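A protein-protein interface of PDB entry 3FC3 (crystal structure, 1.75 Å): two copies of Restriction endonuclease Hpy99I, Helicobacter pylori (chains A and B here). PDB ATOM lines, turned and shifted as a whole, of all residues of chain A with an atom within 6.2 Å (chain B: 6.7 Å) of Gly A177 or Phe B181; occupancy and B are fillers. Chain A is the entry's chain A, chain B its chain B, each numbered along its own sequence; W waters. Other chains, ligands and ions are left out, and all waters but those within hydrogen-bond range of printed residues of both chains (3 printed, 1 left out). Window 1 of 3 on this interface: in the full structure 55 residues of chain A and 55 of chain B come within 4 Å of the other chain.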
ATOM      1  N   ILE A 142     -12.133  10.327   9.814  1.00  0.00           N
ATOM      2  CA  ILE A 142     -11.935  10.459  11.253  1.00  0.00           C
ATOM      3  C   ILE A 142     -12.749   9.397  11.990  1.00  0.00           C
ATOM      4  O   ILE A 142     -12.179   8.499  12.605  1.00  0.00           O
ATOM      5  CB  ILE A 142     -12.256  11.882  11.742  1.00  0.00           C
ATOM      6  CG1 ILE A 142     -11.325  12.900  11.063  1.00  0.00           C
ATOM      7  CG2 ILE A 142     -12.141  11.974  13.275  1.00  0.00           C
ATOM      8  CD1 ILE A 142     -11.616  14.346  11.346  1.00  0.00           C
ATOM      9  N   CYS A 143     -14.080   9.483  11.923  1.00  0.00           N
ATOM     10  CA  CYS A 143     -14.953   8.588  12.674  1.00  0.00           C
ATOM     11  C   CYS A 143     -15.151   7.201  12.044  1.00  0.00           C
ATOM     12  O   CYS A 143     -15.687   6.291  12.694  1.00  0.00           O
ATOM     13  CB  CYS A 143     -16.330   9.226  12.893  1.00  0.00           C
ATOM     14  SG  CYS A 143     -17.307   9.425  11.406  1.00  0.00           S
ATOM     15  N   ASP A 172     -19.952  16.312   8.920  1.00  0.00           N
ATOM     16  CA  ASP A 172     -20.315  17.494   9.698  1.00  0.00           C
ATOM     17  C   ASP A 172     -20.250  17.203  11.203  1.00  0.00           C
ATOM     18  O   ASP A 172     -19.828  18.069  11.996  1.00  0.00           O
ATOM     19  CB  ASP A 172     -21.711  17.975   9.255  1.00  0.00           C
ATOM     20  CG  ASP A 172     -22.201  19.189  10.028  1.00  0.00           C
ATOM     21  OD1 ASP A 172     -21.805  20.329   9.673  1.00  0.00           O
ATOM     22  OD2 ASP A 172     -23.045  19.016  10.941  1.00  0.00           O
ATOM     23  N   SER A 173     -20.630  15.995  11.599  1.00  0.00           N
ATOM     24  CA  SER A 173     -20.517  15.561  12.988  1.00  0.00           C
ATOM     25  C   SER A 173     -19.061  15.684  13.497  1.00  0.00           C
ATOM     26  O   SER A 173     -18.799  16.272  14.548  1.00  0.00           O
ATOM     27  CB  SER A 173     -21.046  14.117  13.088  1.00  0.00           C
ATOM     28  OG  SER A 173     -20.955  13.607  14.396  1.00  0.00           O
ATOM     29  N   CYS A 174     -18.103  15.151  12.746  1.00  0.00           N
ATOM     30  CA  CYS A 174     -16.689  15.251  13.135  1.00  0.00           C
ATOM     31  C   CYS A 174     -16.200  16.685  13.128  1.00  0.00           C
ATOM     32  O   CYS A 174     -15.516  17.121  14.039  1.00  0.00           O
ATOM     33  CB  CYS A 174     -15.816  14.417  12.219  1.00  0.00           C
ATOM     34  SG  CYS A 174     -15.957  12.650  12.631  1.00  0.00           S
ATOM     35  N   ASN A 175     -16.529  17.404  12.071  1.00  0.00           N
ATOM     36  CA  ASN A 175     -16.130  18.810  11.957  1.00  0.00           C
ATOM     37  C   ASN A 175     -16.565  19.642  13.168  1.00  0.00           C
ATOM     38  O   ASN A 175     -15.781  20.426  13.739  1.00  0.00           O
ATOM     39  CB  ASN A 175     -16.686  19.393  10.679  1.00  0.00           C
ATOM     40  CG  ASN A 175     -16.100  20.746  10.359  1.00  0.00           C
ATOM     41  OD1 ASN A 175     -14.880  20.903  10.314  1.00  0.00           O
ATOM     42  ND2 ASN A 175     -16.962  21.736  10.141  1.00  0.00           N
ATOM     43  N   THR A 176     -17.818  19.475  13.557  1.00  0.00           N
ATOM     44  CA  THR A 176     -18.337  20.213  14.693  1.00  0.00           C
ATOM     45  C   THR A 176     -17.819  19.685  16.040  1.00  0.00           C
ATOM     46  O   THR A 176     -17.883  20.411  17.046  1.00  0.00           O
ATOM     47  CB  THR A 176     -19.873  20.303  14.639  1.00  0.00           C
ATOM     48  OG1 THR A 176     -20.452  18.993  14.492  1.00  0.00           O
ATOM     49  CG2 THR A 176     -20.284  21.178  13.451  1.00  0.00           C
ATOM     50  N   GLY A 177     -17.290  18.453  16.046  1.00  0.00           N
ATOM     51  CA  GLY A 177     -16.560  17.896  17.183  1.00  0.00           C
ATOM     52  C   GLY A 177     -15.185  18.521  17.325  1.00  0.00           C
ATOM     53  O   GLY A 177     -14.768  18.919  18.429  1.00  0.00           O
ATOM     54  N   LEU A 178     -14.478  18.662  16.203  1.00  0.00           N
ATOM     55  CA  LEU A 178     -13.172  19.339  16.209  1.00  0.00           C
ATOM     56  C   LEU A 178     -13.291  20.715  16.839  1.00  0.00           C
ATOM     57  O   LEU A 178     -12.475  21.090  17.664  1.00  0.00           O
ATOM     58  CB  LEU A 178     -12.611  19.511  14.794  1.00  0.00           C
ATOM     59  CG  LEU A 178     -12.363  18.270  13.936  1.00  0.00           C
ATOM     60  CD1 LEU A 178     -11.716  18.642  12.592  1.00  0.00           C
ATOM     61  CD2 LEU A 178     -11.533  17.290  14.674  1.00  0.00           C
ATOM     62  N   GLY A 179     -14.323  21.462  16.453  1.00  0.00           N
ATOM     63  CA  GLY A 179     -14.528  22.817  16.988  1.00  0.00           C
ATOM     64  C   GLY A 179     -14.772  22.876  18.485  1.00  0.00           C
ATOM     65  O   GLY A 179     -14.344  23.822  19.154  1.00  0.00           O
ATOM     66  N   ARG A 180     -15.494  21.887  19.012  1.00  0.00           N
ATOM     67  CA  ARG A 180     -15.710  21.836  20.449  1.00  0.00           C
ATOM     68  C   ARG A 180     -14.382  21.775  21.227  1.00  0.00           C
ATOM     69  O   ARG A 180     -14.313  22.226  22.368  1.00  0.00           O
ATOM     70  CB  ARG A 180     -16.606  20.680  20.827  1.00  0.00           C
ATOM     71  CG  ARG A 180     -18.038  20.880  20.413  1.00  0.00           C
ATOM     72  CD  ARG A 180     -18.775  19.544  20.322  1.00  0.00           C
ATOM     73  NE  ARG A 180     -20.180  19.712  20.590  1.00  0.00           N
ATOM     74  CZ  ARG A 180     -21.064  20.254  19.752  1.00  0.00           C
ATOM     75  NH1 ARG A 180     -20.705  20.605  18.543  1.00  0.00           N
ATOM     76  NH2 ARG A 180     -22.332  20.361  20.117  1.00  0.00           N
ATOM     77  N   PHE A 181     -13.352  21.212  20.610  1.00  0.00           N
ATOM     78  CA  PHE A 181     -12.018  21.109  21.223  1.00  0.00           C
ATOM     79  C   PHE A 181     -11.018  22.070  20.560  1.00  0.00           C
ATOM     80  O   PHE A 181      -9.790  21.852  20.617  1.00  0.00           O
ATOM     81  CB  PHE A 181     -11.571  19.639  21.194  1.00  0.00           C
ATOM     82  CG  PHE A 181     -12.582  18.725  21.847  1.00  0.00           C
ATOM     83  CD1 PHE A 181     -12.972  18.957  23.159  1.00  0.00           C
ATOM     84  CD2 PHE A 181     -13.199  17.707  21.145  1.00  0.00           C
ATOM     85  CE1 PHE A 181     -13.936  18.194  23.770  1.00  0.00           C
ATOM     86  CE2 PHE A 181     -14.165  16.918  21.750  1.00  0.00           C
ATOM     87  CZ  PHE A 181     -14.536  17.161  23.083  1.00  0.00           C
ATOM     88  N   LYS A 182     -11.561  23.123  19.929  1.00  0.00           N
ATOM     89  CA  LYS A 182     -10.778  24.256  19.422  1.00  0.00           C
ATOM     90  C   LYS A 182      -9.779  23.865  18.323  1.00  0.00           C
ATOM     91  O   LYS A 182      -8.798  24.583  18.102  1.00  0.00           O
ATOM     92  CB  LYS A 182     -10.051  24.954  20.578  1.00  0.00           C
ATOM     93  CG  LYS A 182     -10.947  25.243  21.777  1.00  0.00           C
ATOM     94  CD  LYS A 182     -10.222  26.018  22.862  1.00  0.00           C
ATOM     95  CE  LYS A 182     -10.857  25.806  24.258  1.00  0.00           C
ATOM     96  NZ  LYS A 182     -10.291  26.713  25.311  1.00  0.00           N
ATOM     97  N   ASP A 183     -10.047  22.755  17.632  1.00  0.00           N
ATOM     98  CA  ASP A 183      -9.136  22.223  16.592  1.00  0.00           C
ATOM     99  C   ASP A 183      -7.721  22.082  17.159  1.00  0.00           C
ATOM    100  O   ASP A 183      -6.732  22.186  16.421  1.00  0.00           O
ATOM    101  CB  ASP A 183      -9.062  23.132  15.350  1.00  0.00           C
ATOM    102  CG  ASP A 183     -10.347  23.192  14.546  1.00  0.00           C
ATOM    103  OD1 ASP A 183     -11.430  22.718  14.979  1.00  0.00           O
ATOM    104  OD2 ASP A 183     -10.260  23.777  13.441  1.00  0.00           O
ATOM    105  N   LEU A 188      -7.703  17.608  22.826  1.00  0.00           N
ATOM    106  CA  LEU A 188      -7.993  16.221  22.480  1.00  0.00           C
ATOM    107  C   LEU A 188      -7.214  15.296  23.411  1.00  0.00           C
ATOM    108  O   LEU A 188      -7.720  14.260  23.851  1.00  0.00           O
ATOM    109  CB  LEU A 188      -7.640  15.952  21.016  1.00  0.00           C
ATOM    110  CG  LEU A 188      -8.487  16.747  20.014  1.00  0.00           C
ATOM    111  CD1 LEU A 188      -7.863  16.635  18.646  1.00  0.00           C
ATOM    112  CD2 LEU A 188      -9.933  16.263  20.015  1.00  0.00           C
ATOM    113  N   THR B 176     -21.053  16.650  24.282  1.00  0.00           N
ATOM    114  CA  THR B 176     -21.598  16.333  22.958  1.00  0.00           C
ATOM    115  C   THR B 176     -20.493  16.138  21.930  1.00  0.00           C
ATOM    116  O   THR B 176     -20.722  15.537  20.873  1.00  0.00           O
ATOM    117  CB  THR B 176     -22.649  17.375  22.507  1.00  0.00           C
ATOM    118  OG1 THR B 176     -22.173  18.745  22.654  1.00  0.00           O
ATOM    119  CG2 THR B 176     -23.883  17.214  23.373  1.00  0.00           C
ATOM    120  N   GLY B 177     -19.318  16.679  22.237  1.00  0.00           N
ATOM    121  CA  GLY B 177     -18.091  16.387  21.504  1.00  0.00           C
ATOM    122  C   GLY B 177     -17.580  14.978  21.735  1.00  0.00           C
ATOM    123  O   GLY B 177     -17.220  14.276  20.780  1.00  0.00           O
ATOM    124  N   LEU B 178     -17.532  14.551  22.993  1.00  0.00           N
ATOM    125  CA  LEU B 178     -17.152  13.192  23.308  1.00  0.00           C
ATOM    126  C   LEU B 178     -17.955  12.199  22.483  1.00  0.00           C
ATOM    127  O   LEU B 178     -17.396  11.244  21.921  1.00  0.00           O
ATOM    128  CB  LEU B 178     -17.351  12.881  24.784  1.00  0.00           C
ATOM    129  CG  LEU B 178     -16.491  13.590  25.829  1.00  0.00           C
ATOM    130  CD1 LEU B 178     -16.730  13.008  27.225  1.00  0.00           C
ATOM    131  CD2 LEU B 178     -15.048  13.542  25.452  1.00  0.00           C
ATOM    132  N   GLY B 179     -19.261  12.425  22.400  1.00  0.00           N
ATOM    133  CA  GLY B 179     -20.175  11.539  21.671  1.00  0.00           C
ATOM    134  C   GLY B 179     -19.916  11.427  20.185  1.00  0.00           C
ATOM    135  O   GLY B 179     -20.080  10.349  19.601  1.00  0.00           O
ATOM    136  N   ARG B 180     -19.509  12.535  19.569  1.00  0.00           N
ATOM    137  CA  ARG B 180     -19.118  12.534  18.157  1.00  0.00           C
ATOM    138  C   ARG B 180     -17.945  11.570  17.877  1.00  0.00           C
ATOM    139  O   ARG B 180     -17.834  11.005  16.775  1.00  0.00           O
ATOM    140  CB  ARG B 180     -18.775  13.953  17.708  1.00  0.00           C
ATOM    141  CG  ARG B 180     -20.000  14.878  17.621  1.00  0.00           C
ATOM    142  CD  ARG B 180     -19.585  16.318  17.585  1.00  0.00           C
ATOM    143  NE  ARG B 180     -20.557  17.128  16.862  1.00  0.00           N
ATOM    144  CZ  ARG B 180     -21.740  17.500  17.314  1.00  0.00           C
ATOM    145  NH1 ARG B 180     -22.134  17.176  18.523  1.00  0.00           N
ATOM    146  NH2 ARG B 180     -22.531  18.252  16.543  1.00  0.00           N
ATOM    147  N   PHE B 181     -17.119  11.352  18.884  1.00  0.00           N
ATOM    148  CA  PHE B 181     -15.985  10.438  18.761  1.00  0.00           C
ATOM    149  C   PHE B 181     -16.203   9.164  19.583  1.00  0.00           C
ATOM    150  O   PHE B 181     -15.250   8.458  19.943  1.00  0.00           O
ATOM    151  CB  PHE B 181     -14.696  11.193  19.100  1.00  0.00           C
ATOM    152  CG  PHE B 181     -14.536  12.437  18.286  1.00  0.00           C
ATOM    153  CD1 PHE B 181     -14.508  12.362  16.899  1.00  0.00           C
ATOM    154  CD2 PHE B 181     -14.488  13.685  18.883  1.00  0.00           C
ATOM    155  CE1 PHE B 181     -14.440  13.508  16.134  1.00  0.00           C
ATOM    156  CE2 PHE B 181     -14.393  14.825  18.118  1.00  0.00           C
ATOM    157  CZ  PHE B 181     -14.361  14.738  16.751  1.00  0.00           C
ATOM    158  N   LYS B 182     -17.477   8.850  19.812  1.00  0.00           N
ATOM    159  CA  LYS B 182     -17.915   7.589  20.415  1.00  0.00           C
ATOM    160  C   LYS B 182     -17.364   7.324  21.835  1.00  0.00           C
ATOM    161  O   LYS B 182     -17.310   6.177  22.276  1.00  0.00           O
ATOM    162  CB  LYS B 182     -17.613   6.420  19.465  1.00  0.00           C
ATOM    163  CG  LYS B 182     -17.998   6.700  17.992  1.00  0.00           C
ATOM    164  CD  LYS B 182     -17.779   5.491  17.092  1.00  0.00           C
ATOM    165  CE  LYS B 182     -17.543   5.890  15.616  1.00  0.00           C
ATOM    166  NZ  LYS B 182     -17.470   4.691  14.724  1.00  0.00           N
ATOM    167  N   ASP B 183     -17.009   8.394  22.549  1.00  0.00           N
ATOM    168  CA  ASP B 183     -16.358   8.317  23.872  1.00  0.00           C
ATOM    169  C   ASP B 183     -15.135   7.372  23.830  1.00  0.00           C
ATOM    170  O   ASP B 183     -14.827   6.705  24.826  1.00  0.00           O
ATOM    171  CB  ASP B 183     -17.324   7.796  24.967  1.00  0.00           C
ATOM    172  CG  ASP B 183     -18.464   8.747  25.332  1.00  0.00           C
ATOM    173  OD1 ASP B 183     -18.756   9.785  24.635  1.00  0.00           O
ATOM    174  OD2 ASP B 183     -19.092   8.402  26.361  1.00  0.00           O
ATOM    175  N   ASN B 184     -14.447   7.320  22.691  1.00  0.00           N
ATOM    176  CA  ASN B 184     -13.428   6.298  22.422  1.00  0.00           C
ATOM    177  C   ASN B 184     -12.081   6.945  22.110  1.00  0.00           C
ATOM    178  O   ASN B 184     -11.927   7.611  21.097  1.00  0.00           O
ATOM    179  CB  ASN B 184     -13.877   5.401  21.252  1.00  0.00           C
ATOM    180  CG  ASN B 184     -12.994   4.162  21.050  1.00  0.00           C
ATOM    181  OD1 ASN B 184     -11.845   4.111  21.468  1.00  0.00           O
ATOM    182  ND2 ASN B 184     -13.551   3.162  20.389  1.00  0.00           N
ATOM    183  N   PRO B 185     -11.072   6.706  22.959  1.00  0.00           N
ATOM    184  CA  PRO B 185      -9.731   7.268  22.693  1.00  0.00           C
ATOM    185  C   PRO B 185      -9.149   6.940  21.305  1.00  0.00           C
ATOM    186  O   PRO B 185      -8.311   7.688  20.806  1.00  0.00           O
ATOM    187  CB  PRO B 185      -8.856   6.631  23.785  1.00  0.00           C
ATOM    188  CG  PRO B 185      -9.802   6.278  24.886  1.00  0.00           C
ATOM    189  CD  PRO B 185     -11.100   5.903  24.199  1.00  0.00           C
ATOM    190  N   LYS B 186      -9.575   5.838  20.704  1.00  0.00           N
ATOM    191  CA  LYS B 186      -9.155   5.476  19.349  1.00  0.00           C
ATOM    192  C   LYS B 186      -9.433   6.593  18.345  1.00  0.00           C
ATOM    193  O   LYS B 186      -8.556   6.979  17.560  1.00  0.00           O
ATOM    194  CB  LYS B 186      -9.883   4.214  18.897  1.00  0.00           C
ATOM    195  CG  LYS B 186      -9.623   3.825  17.451  1.00  0.00           C
ATOM    196  CD  LYS B 186     -10.518   2.696  16.998  1.00  0.00           C
ATOM    197  CE  LYS B 186     -10.520   2.596  15.486  1.00  0.00           C
ATOM    198  NZ  LYS B 186     -10.781   1.195  15.041  1.00  0.00           N
ATOM    199  N   PHE B 187     -10.661   7.104  18.365  1.00  0.00           N
ATOM    200  CA  PHE B 187     -11.043   8.143  17.420  1.00  0.00           C
ATOM    201  C   PHE B 187     -10.466   9.472  17.803  1.00  0.00           C
ATOM    202  O   PHE B 187     -10.172  10.279  16.934  1.00  0.00           O
ATOM    203  CB  PHE B 187     -12.554   8.182  17.242  1.00  0.00           C
ATOM    204  CG  PHE B 187     -13.083   6.906  16.708  1.00  0.00           C
ATOM    205  CD1 PHE B 187     -12.779   6.524  15.406  1.00  0.00           C
ATOM    206  CD2 PHE B 187     -13.785   6.028  17.517  1.00  0.00           C
ATOM    207  CE1 PHE B 187     -13.208   5.314  14.908  1.00  0.00           C
ATOM    208  CE2 PHE B 187     -14.236   4.811  17.015  1.00  0.00           C
ATOM    209  CZ  PHE B 187     -13.941   4.456  15.706  1.00  0.00           C
ATOM    210  N   LEU B 188     -10.278   9.702  19.097  1.00  0.00           N
ATOM    211  CA  LEU B 188      -9.615  10.923  19.543  1.00  0.00           C
ATOM    212  C   LEU B 188      -8.156  10.955  19.068  1.00  0.00           C
ATOM    213  O   LEU B 188      -7.652  11.993  18.651  1.00  0.00           O
ATOM    214  CB  LEU B 188      -9.729  11.076  21.063  1.00  0.00           C
ATOM    215  CG  LEU B 188     -11.195  11.241  21.521  1.00  0.00           C
ATOM    216  CD1 LEU B 188     -11.354  10.810  22.954  1.00  0.00           C
ATOM    217  CD2 LEU B 188     -11.668  12.650  21.315  1.00  0.00           C
ATOM    218  N   VAL B 191      -8.204  11.950  15.479  1.00  0.00           N
ATOM    219  CA  VAL B 191      -8.363  13.395  15.356  1.00  0.00           C
ATOM    220  C   VAL B 191      -7.003  14.072  15.528  1.00  0.00           C
ATOM    221  O   VAL B 191      -6.637  14.946  14.746  1.00  0.00           O
ATOM    222  CB  VAL B 191      -9.352  13.947  16.406  1.00  0.00           C
ATOM    223  CG1 VAL B 191      -9.402  15.456  16.356  1.00  0.00           C
ATOM    224  CG2 VAL B 191     -10.736  13.351  16.189  1.00  0.00           C
HETATM  225  O   HOH W   1     -18.717  12.017  14.367  1.00  0.00           O
HETATM  226  O   HOH W   2     -23.356  21.811  23.009  1.00  0.00           O
HETATM  227  O   HOH W   3     -23.226  17.510  13.358  1.00  0.00           O
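NZ of Lys B182 is in hydrogen-bond range of O of Cys A143, at 3.1 Å. O of Ser A173 is in hydrogen-bond range of NE of Arg B180, 3.0 Å away. The side-chain hydroxyl (OG1) of Thr A176 is in hydrogen-bond range of the guanidinium group (NH2) of Arg B180, at 3.0 Å. The guanidinium group (NH2) of Arg A180 is in hydrogen-bond range of the side-chain hydroxyl (OG1) of Thr B176.
Thr A176 touches Arg B180, and with the chains exchanged Arg A180 touches Thr B176. Gly A177 touches Arg B180, and with the chains exchanged Arg A180 touches Gly B177. Leu A178 touches Phe B181, and with the chains exchanged Phe A181 touches Leu B178. Arg A180 touches its own counterpart, Arg B180. Positions printed for both chains: 176, 177, 178, 179, 180, 181, 182, 183 and 188. Of the 18 pairs that touch across the chains among the printed residues, 9 have their exchanged pair printed and touching as well.
Water W1 bridges the side-chain hydroxyl (OG) of Ser A173 and the backbone carbonyl oxygen (O) of Arg B180. Water W3 lies within hydrogen-bond range of OD2 of Asp A172 (2.9 Å), OG1 of Thr A176 (3.3 Å), NH2 of Arg B180 (3.3 Å) and N of Ser A173 (3.5 Å). Water W2 bridges the side-chain hydroxyl (OG1) of Thr B176 and the guanidinium group (NH2) of Arg A180.
OG1 of Thr A176 is in hydrogen-bond range of O of Asp A172, at 2.7 Å. OG1 of Thr A176 sits at hydrogen-bond distance from O of Ser A173 (3.2 Å). The backbone carbonyl oxygen of Thr A176 sits at hydrogen-bond distance from the guanidinium group of Arg A180, at 3.2 Å. The backbone NH (N) of Asp A183 sits at hydrogen-bond distance from the backbone carbonyl oxygen (O) of Leu A178 (2.9 Å). The backbone carbonyl oxygen of Thr B176 is in hydrogen-bond range of the guanidinium group of Arg B180. The backbone carbonyl oxygen (O) of Leu B178 sits at hydrogen-bond distance from the backbone NH (N) of Asp B183 (2.9 Å).
Along chain A the printed residues that touch a printed residue of chain B span positions 142 to 188.
Among the printed residues, pairs that only touch across the chains: Ile A142 with Phe B181, Ile A142 with Phe B187, Ile A142 with Val B191, Cys A143 with Phe B187, Cys A174 with Phe B181, Gly A177 with Arg B180, Gly A177 with Phe B181, Leu A178 with Phe B181, Leu A178 with Val B191, Arg A180 with Gly B177, Arg A180 with Arg B180, Phe A181 with Gly B177, Phe A181 with Leu B178 and Leu A188 with Val B191.
Of chain B, only Arg B180 (3.4 Å) and Phe B181 (3.9 Å) come within 4 Å of Gly A177. Phe B181 touches just these residues of chain A: Ile A142, Cys A174, Gly A177 and Leu A178. Printed residues of chain A within 4 Å of Lys B182: Cys A143 (3.1 Å). Of the printed residues of chain A, Thr B176 touches Arg A180 (3.0 Å). Of the printed residues of chain B, Leu A178 touches Phe B181 (3.96 Å) and Val B191 (3.3 Å). Of the printed residues of chain B, Phe A181 touches Gly B177 and Leu B178. Leu B188 touches none of the printed residues of chain A. The nearest residue of chain B that does not touch Gly A177 is Gly B177 (4.8 Å). The nearest residue of chain A that does not touch Phe B181 is Phe A181 (4.2 Å). The nearest printed residue of chain B that does not touch Leu A178 is Arg B180 (5.8 Å).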
